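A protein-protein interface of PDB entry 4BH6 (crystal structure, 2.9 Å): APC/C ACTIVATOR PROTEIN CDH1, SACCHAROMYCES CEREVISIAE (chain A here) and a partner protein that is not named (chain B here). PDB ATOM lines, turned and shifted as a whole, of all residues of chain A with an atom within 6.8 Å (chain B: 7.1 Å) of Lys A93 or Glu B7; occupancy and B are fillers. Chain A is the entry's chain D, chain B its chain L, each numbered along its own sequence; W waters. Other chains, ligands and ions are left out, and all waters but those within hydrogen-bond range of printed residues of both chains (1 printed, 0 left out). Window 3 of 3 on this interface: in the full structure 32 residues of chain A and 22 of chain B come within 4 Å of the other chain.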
ATOM      1  N   SER A  75     -24.265  -5.682 -26.620  1.00  0.00           N
ATOM      2  CA  SER A  75     -23.755  -6.797 -25.804  1.00  0.00           C
ATOM      3  C   SER A  75     -24.616  -8.073 -25.884  1.00  0.00           C
ATOM      4  O   SER A  75     -24.119  -9.179 -25.658  1.00  0.00           O
ATOM      5  CB  SER A  75     -23.625  -6.359 -24.334  1.00  0.00           C
ATOM      6  OG  SER A  75     -24.873  -5.968 -23.783  1.00  0.00           O
ATOM      7  N   HIS A  76     -25.910  -7.912 -26.177  1.00  0.00           N
ATOM      8  CA  HIS A  76     -26.867  -9.021 -26.181  1.00  0.00           C
ATOM      9  C   HIS A  76     -27.702  -9.024 -27.448  1.00  0.00           C
ATOM     10  O   HIS A  76     -28.059  -7.964 -27.972  1.00  0.00           O
ATOM     11  CB  HIS A  76     -27.797  -8.935 -24.975  1.00  0.00           C
ATOM     12  CG  HIS A  76     -27.091  -9.041 -23.662  1.00  0.00           C
ATOM     13  ND1 HIS A  76     -26.949 -10.237 -22.996  1.00  0.00           N
ATOM     14  CD2 HIS A  76     -26.491  -8.102 -22.890  1.00  0.00           C
ATOM     15  CE1 HIS A  76     -26.286 -10.033 -21.872  1.00  0.00           C
ATOM     16  NE2 HIS A  76     -26.001  -8.745 -21.782  1.00  0.00           N
ATOM     17  N   ASP A  90     -26.169 -13.685 -24.435  1.00  0.00           N
ATOM     18  CA  ASP A  90     -24.946 -12.953 -24.106  1.00  0.00           C
ATOM     19  C   ASP A  90     -23.926 -13.335 -25.154  1.00  0.00           C
ATOM     20  O   ASP A  90     -23.461 -14.479 -25.192  1.00  0.00           O
ATOM     21  CB  ASP A  90     -24.406 -13.278 -22.709  1.00  0.00           C
ATOM     22  CG  ASP A  90     -23.250 -12.336 -22.282  1.00  0.00           C
ATOM     23  OD1 ASP A  90     -22.333 -12.071 -23.100  1.00  0.00           O
ATOM     24  OD2 ASP A  90     -23.247 -11.860 -21.116  1.00  0.00           O
ATOM     25  N   VAL A  91     -23.598 -12.365 -26.001  1.00  0.00           N
ATOM     26  CA  VAL A  91     -22.746 -12.576 -27.159  1.00  0.00           C
ATOM     27  C   VAL A  91     -21.262 -12.850 -26.780  1.00  0.00           C
ATOM     28  O   VAL A  91     -20.593 -13.686 -27.396  1.00  0.00           O
ATOM     29  CB  VAL A  91     -22.958 -11.414 -28.150  1.00  0.00           C
ATOM     30  CG1 VAL A  91     -21.684 -11.048 -28.900  1.00  0.00           C
ATOM     31  CG2 VAL A  91     -24.089 -11.761 -29.103  1.00  0.00           C
ATOM     32  N   MET A  92     -20.767 -12.171 -25.748  1.00  0.00           N
ATOM     33  CA  MET A  92     -19.415 -12.398 -25.272  1.00  0.00           C
ATOM     34  C   MET A  92     -19.298 -13.794 -24.657  1.00  0.00           C
ATOM     35  O   MET A  92     -18.337 -14.521 -24.935  1.00  0.00           O
ATOM     36  CB  MET A  92     -19.042 -11.351 -24.237  1.00  0.00           C
ATOM     37  CG  MET A  92     -19.413  -9.930 -24.604  1.00  0.00           C
ATOM     38  SD  MET A  92     -17.901  -9.148 -25.182  1.00  0.00           S
ATOM     39  CE  MET A  92     -16.990  -8.910 -23.646  1.00  0.00           C
ATOM     40  N   LYS A  93     -20.279 -14.159 -23.824  1.00  0.00           N
ATOM     41  CA  LYS A  93     -20.353 -15.485 -23.180  1.00  0.00           C
ATOM     42  C   LYS A  93     -20.772 -16.610 -24.148  1.00  0.00           C
ATOM     43  O   LYS A  93     -20.504 -17.781 -23.907  1.00  0.00           O
ATOM     44  CB  LYS A  93     -21.368 -15.454 -22.041  1.00  0.00           C
ATOM     45  CG  LYS A  93     -20.861 -15.180 -20.639  1.00  0.00           C
ATOM     46  CD  LYS A  93     -21.991 -15.557 -19.677  1.00  0.00           C
ATOM     47  CE  LYS A  93     -22.155 -14.584 -18.519  1.00  0.00           C
ATOM     48  NZ  LYS A  93     -21.037 -14.718 -17.545  1.00  0.00           N
ATOM     49  N   ARG A  94     -21.456 -16.247 -25.228  1.00  0.00           N
ATOM     50  CA  ARG A  94     -22.019 -17.216 -26.179  1.00  0.00           C
ATOM     51  C   ARG A  94     -23.024 -18.169 -25.527  1.00  0.00           C
ATOM     52  O   ARG A  94     -23.145 -19.316 -25.927  1.00  0.00           O
ATOM     53  CB  ARG A  94     -20.916 -17.988 -26.923  1.00  0.00           C
ATOM     54  CG  ARG A  94     -19.983 -17.093 -27.707  1.00  0.00           C
ATOM     55  CD  ARG A  94     -19.151 -17.886 -28.693  1.00  0.00           C
ATOM     56  NE  ARG A  94     -18.008 -17.102 -29.170  1.00  0.00           N
ATOM     57  CZ  ARG A  94     -17.000 -17.593 -29.881  1.00  0.00           C
ATOM     58  NH1 ARG A  94     -16.984 -18.873 -30.226  1.00  0.00           N
ATOM     59  NH2 ARG A  94     -16.011 -16.798 -30.262  1.00  0.00           N
ATOM     60  N   LYS A  95     -23.736 -17.684 -24.521  1.00  0.00           N
ATOM     61  CA  LYS A  95     -24.711 -18.487 -23.797  1.00  0.00           C
ATOM     62  C   LYS A  95     -26.099 -17.830 -23.909  1.00  0.00           C
ATOM     63  O   LYS A  95     -26.209 -16.613 -24.118  1.00  0.00           O
ATOM     64  CB  LYS A  95     -24.283 -18.641 -22.333  1.00  0.00           C
ATOM     65  N   CYS A  96     -27.158 -18.625 -23.785  1.00  0.00           N
ATOM     66  CA  CYS A  96     -28.511 -18.071 -23.771  1.00  0.00           C
ATOM     67  C   CYS A  96     -28.865 -17.598 -22.361  1.00  0.00           C
ATOM     68  O   CYS A  96     -29.111 -18.399 -21.453  1.00  0.00           O
ATOM     69  CB  CYS A  96     -29.539 -19.077 -24.286  1.00  0.00           C
ATOM     70  SG  CYS A  96     -31.268 -18.569 -24.078  1.00  0.00           S
ATOM     71  N   ILE A  97     -28.891 -16.282 -22.206  1.00  0.00           N
ATOM     72  CA  ILE A  97     -29.109 -15.617 -20.936  1.00  0.00           C
ATOM     73  C   ILE A  97     -30.505 -15.814 -20.370  1.00  0.00           C
ATOM     74  O   ILE A  97     -30.654 -15.929 -19.139  1.00  0.00           O
ATOM     75  CB  ILE A  97     -28.707 -14.112 -21.053  1.00  0.00           C
ATOM     76  CG1 ILE A  97     -27.229 -13.964 -20.655  1.00  0.00           C
ATOM     77  CG2 ILE A  97     -29.629 -13.146 -20.284  1.00  0.00           C
ATOM     78  CD1 ILE A  97     -26.765 -14.945 -19.596  1.00  0.00           C
ATOM     79  N   ARG A  98     -31.514 -15.824 -21.252  1.00  0.00           N
ATOM     80  CA  ARG A  98     -32.904 -16.098 -20.840  1.00  0.00           C
ATOM     81  C   ARG A  98     -33.916 -16.448 -21.929  1.00  0.00           C
ATOM     82  O   ARG A  98     -33.715 -16.151 -23.101  1.00  0.00           O
ATOM     83  CB  ARG A  98     -33.446 -15.063 -19.834  1.00  0.00           C
ATOM     84  CG  ARG A  98     -33.962 -13.760 -20.367  1.00  0.00           C
ATOM     85  CD  ARG A  98     -34.517 -12.969 -19.192  1.00  0.00           C
ATOM     86  NE  ARG A  98     -35.581 -13.701 -18.495  1.00  0.00           N
ATOM     87  CZ  ARG A  98     -36.600 -13.106 -17.877  1.00  0.00           C
ATOM     88  NH1 ARG A  98     -36.699 -11.781 -17.886  1.00  0.00           N
ATOM     89  NH2 ARG A  98     -37.538 -13.828 -17.273  1.00  0.00           N
ATOM     90  N   VAL A 131     -36.462  -6.462 -19.174  1.00  0.00           N
ATOM     91  CA  VAL A 131     -35.448  -7.461 -19.354  1.00  0.00           C
ATOM     92  C   VAL A 131     -34.568  -7.698 -18.124  1.00  0.00           C
ATOM     93  O   VAL A 131     -33.766  -8.657 -18.101  1.00  0.00           O
ATOM     94  CB  VAL A 131     -34.640  -7.088 -20.575  1.00  0.00           C
ATOM     95  CG1 VAL A 131     -33.278  -6.544 -20.201  1.00  0.00           C
ATOM     96  CG2 VAL A 131     -34.557  -8.264 -21.509  1.00  0.00           C
ATOM     97  N   ARG A 132     -34.725  -6.841 -17.106  1.00  0.00           N
ATOM     98  CA  ARG A 132     -34.050  -6.989 -15.811  1.00  0.00           C
ATOM     99  C   ARG A 132     -34.952  -7.736 -14.865  1.00  0.00           C
ATOM    100  O   ARG A 132     -34.532  -8.154 -13.803  1.00  0.00           O
ATOM    101  CB  ARG A 132     -33.790  -5.633 -15.185  1.00  0.00           C
ATOM    102  CG  ARG A 132     -33.220  -4.608 -16.126  1.00  0.00           C
ATOM    103  CD  ARG A 132     -33.435  -3.210 -15.574  1.00  0.00           C
ATOM    104  NE  ARG A 132     -34.835  -2.798 -15.631  1.00  0.00           N
ATOM    105  CZ  ARG A 132     -35.285  -1.654 -15.138  1.00  0.00           C
ATOM    106  NH1 ARG A 132     -34.454  -0.818 -14.530  1.00  0.00           N
ATOM    107  NH2 ARG A 132     -36.569  -1.360 -15.224  1.00  0.00           N
ATOM    108  N   MET B   4     -28.352  -4.182 -15.754  1.00  0.00           N
ATOM    109  CA  MET B   4     -28.120  -5.605 -15.426  1.00  0.00           C
ATOM    110  C   MET B   4     -29.178  -6.545 -15.965  1.00  0.00           C
ATOM    111  O   MET B   4     -30.253  -6.631 -15.403  1.00  0.00           O
ATOM    112  CB  MET B   4     -28.110  -5.768 -13.918  1.00  0.00           C
ATOM    113  CG  MET B   4     -26.772  -5.515 -13.268  1.00  0.00           C
ATOM    114  SD  MET B   4     -25.714  -6.959 -13.382  1.00  0.00           S
ATOM    115  CE  MET B   4     -26.481  -8.120 -12.235  1.00  0.00           C
ATOM    116  N   LEU B   5     -28.875  -7.276 -17.027  1.00  0.00           N
ATOM    117  CA  LEU B   5     -29.842  -8.215 -17.600  1.00  0.00           C
ATOM    118  C   LEU B   5     -30.131  -9.302 -16.603  1.00  0.00           C
ATOM    119  O   LEU B   5     -29.206  -9.796 -15.980  1.00  0.00           O
ATOM    120  CB  LEU B   5     -29.269  -8.900 -18.823  1.00  0.00           C
ATOM    121  CG  LEU B   5     -29.294  -8.377 -20.262  1.00  0.00           C
ATOM    122  CD1 LEU B   5     -30.607  -8.734 -20.938  1.00  0.00           C
ATOM    123  CD2 LEU B   5     -28.954  -6.900 -20.338  1.00  0.00           C
ATOM    124  N   TYR B   6     -31.400  -9.688 -16.460  1.00  0.00           N
ATOM    125  CA  TYR B   6     -31.776 -10.774 -15.546  1.00  0.00           C
ATOM    126  C   TYR B   6     -31.373 -12.122 -16.129  1.00  0.00           C
ATOM    127  O   TYR B   6     -31.743 -12.447 -17.261  1.00  0.00           O
ATOM    128  CB  TYR B   6     -33.281 -10.764 -15.238  1.00  0.00           C
ATOM    129  CG  TYR B   6     -33.719 -11.866 -14.278  1.00  0.00           C
ATOM    130  CD1 TYR B   6     -33.621 -11.701 -12.883  1.00  0.00           C
ATOM    131  CD2 TYR B   6     -34.214 -13.079 -14.760  1.00  0.00           C
ATOM    132  CE1 TYR B   6     -34.004 -12.708 -12.004  1.00  0.00           C
ATOM    133  CE2 TYR B   6     -34.597 -14.095 -13.886  1.00  0.00           C
ATOM    134  CZ  TYR B   6     -34.493 -13.903 -12.506  1.00  0.00           C
ATOM    135  OH  TYR B   6     -34.869 -14.893 -11.621  1.00  0.00           O
ATOM    136  N   GLU B   7     -30.637 -12.911 -15.345  1.00  0.00           N
ATOM    137  CA  GLU B   7     -30.065 -14.164 -15.843  1.00  0.00           C
ATOM    138  C   GLU B   7     -30.708 -15.422 -15.250  1.00  0.00           C
ATOM    139  O   GLU B   7     -30.800 -15.590 -14.024  1.00  0.00           O
ATOM    140  CB  GLU B   7     -28.538 -14.169 -15.690  1.00  0.00           C
ATOM    141  CG  GLU B   7     -27.840 -13.135 -16.575  1.00  0.00           C
ATOM    142  CD  GLU B   7     -26.326 -13.089 -16.413  1.00  0.00           C
ATOM    143  OE1 GLU B   7     -25.651 -14.121 -16.654  1.00  0.00           O
ATOM    144  OE2 GLU B   7     -25.805 -12.002 -16.064  1.00  0.00           O
ATOM    145  N   GLU B   8     -31.151 -16.293 -16.160  1.00  0.00           N
ATOM    146  CA  GLU B   8     -31.868 -17.524 -15.836  1.00  0.00           C
ATOM    147  C   GLU B   8     -30.983 -18.607 -15.269  1.00  0.00           C
ATOM    148  O   GLU B   8     -29.872 -18.810 -15.757  1.00  0.00           O
ATOM    149  CB  GLU B   8     -32.439 -18.112 -17.101  1.00  0.00           C
ATOM    150  CG  GLU B   8     -33.886 -17.810 -17.338  1.00  0.00           C
ATOM    151  CD  GLU B   8     -34.331 -18.325 -18.689  1.00  0.00           C
ATOM    152  OE1 GLU B   8     -33.516 -19.022 -19.367  1.00  0.00           O
ATOM    153  OE2 GLU B   8     -35.489 -18.008 -19.067  1.00  0.00           O
ATOM    154  N   THR B   9     -31.485 -19.331 -14.268  1.00  0.00           N
ATOM    155  CA  THR B   9     -30.853 -20.589 -13.867  1.00  0.00           C
ATOM    156  C   THR B   9     -31.295 -21.655 -14.871  1.00  0.00           C
ATOM    157  O   THR B   9     -32.307 -21.482 -15.548  1.00  0.00           O
ATOM    158  CB  THR B   9     -31.174 -21.000 -12.405  1.00  0.00           C
ATOM    159  OG1 THR B   9     -32.528 -21.452 -12.296  1.00  0.00           O
ATOM    160  CG2 THR B   9     -30.964 -19.839 -11.469  1.00  0.00           C
ATOM    161  N   GLU B  12     -34.845 -22.632 -14.165  1.00  0.00           N
ATOM    162  CA  GLU B  12     -35.784 -21.585 -14.580  1.00  0.00           C
ATOM    163  C   GLU B  12     -36.165 -21.675 -16.057  1.00  0.00           C
ATOM    164  O   GLU B  12     -37.347 -21.548 -16.403  1.00  0.00           O
ATOM    165  CB  GLU B  12     -35.205 -20.207 -14.285  1.00  0.00           C
ATOM    166  CG  GLU B  12     -35.318 -19.786 -12.838  1.00  0.00           C
ATOM    167  CD  GLU B  12     -35.098 -18.306 -12.681  1.00  0.00           C
ATOM    168  OE1 GLU B  12     -33.966 -17.856 -12.973  1.00  0.00           O
ATOM    169  OE2 GLU B  12     -36.064 -17.598 -12.288  1.00  0.00           O
HETATM  170  O   HOH W   1     -37.864 -16.785 -17.121  1.00  0.00           O
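O of Val A131 is in hydrogen-bond range of N of Tyr B6 (3.1 Å).
N of Glu B8 sits at hydrogen-bond distance from O of Ile A97, 3.0 Å away.
N of Lys A93 lies within hydrogen-bond range of OD1 of Asp A90, 3.0 Å away.
SG of Cys A96 is in hydrogen-bond range of O of Arg A98 (3.6 Å).
OE2 of Glu B12 is in hydrogen-bond range of OH of Tyr B6.
His A76 touches Leu B5 (NE2 to CG, 3.6 Å).
OE1 of Glu B7 touches CE of Lys A93 (3.99 Å).
Tyr B6 touches Ile A97 (O to CG2, 3.8 Å).
Glu B7 touches Ile A97 (OE1 to CD1, 3.3 Å).
Arg A98 touches Tyr B6.
Arg A98 touches Glu B8.
Leu B5 touches Val A131 (CD1 to CG1, 3.5 Å).
Arg A132 touches Met B4.
Tyr B6 touches Arg A132 (CB to O, 3.2 Å).
Printed residues of chain B within 4 Å of His A76: Leu B5 (3.6 Å).
Of the printed residues of chain B, Lys A93 touches Glu B7.
Of the printed residues of chain A, Met B4 touches Arg A132 (3.7 Å).
Of the printed residues of chain A, Tyr B6 touches Ile A97 (3.8 Å), Arg A98 (3.4 Å), Val A131 (3.1 Å) and Arg A132 (3.2 Å).
Of the printed residues of chain A, Glu B7 touches Lys A93 (3.99 Å) and Ile A97 (3.3 Å).
Of the printed residues of chain A, Glu B8 touches Ile A97 and Arg A98.
The nearest printed residue of chain B that does not touch Lys A93 is Leu B5 (8.9 Å).
Of the 7 printed residues of chain B, 5 touch a printed residue of chain A.
Printed residues of chain B that touch a printed residue of chain A: Met B4, Leu B5, Tyr B6, Glu B7 and Glu B8.
Hydrophobic or aromatic side chains of chain B that line the printed part of chain A: Leu B5 and Tyr B6.
Along chain B the printed residues that touch a printed residue of chain A span positions 4 to 8.
Hydrophobic or aromatic side chains of chain A that line the printed part of chain B: His A76, Ile A97 and Val A131.
Among the printed residues, 11 pairs touch across the chains.
Among the printed residues, no Asp or Glu carboxylate lies within 4 Å of a Lys or Arg side-chain nitrogen of the other chain.
Water W1 lies within hydrogen-bond range of NH2 of Arg A98 (3.0 Å) and OE2 of Glu B8 (3.3 Å).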
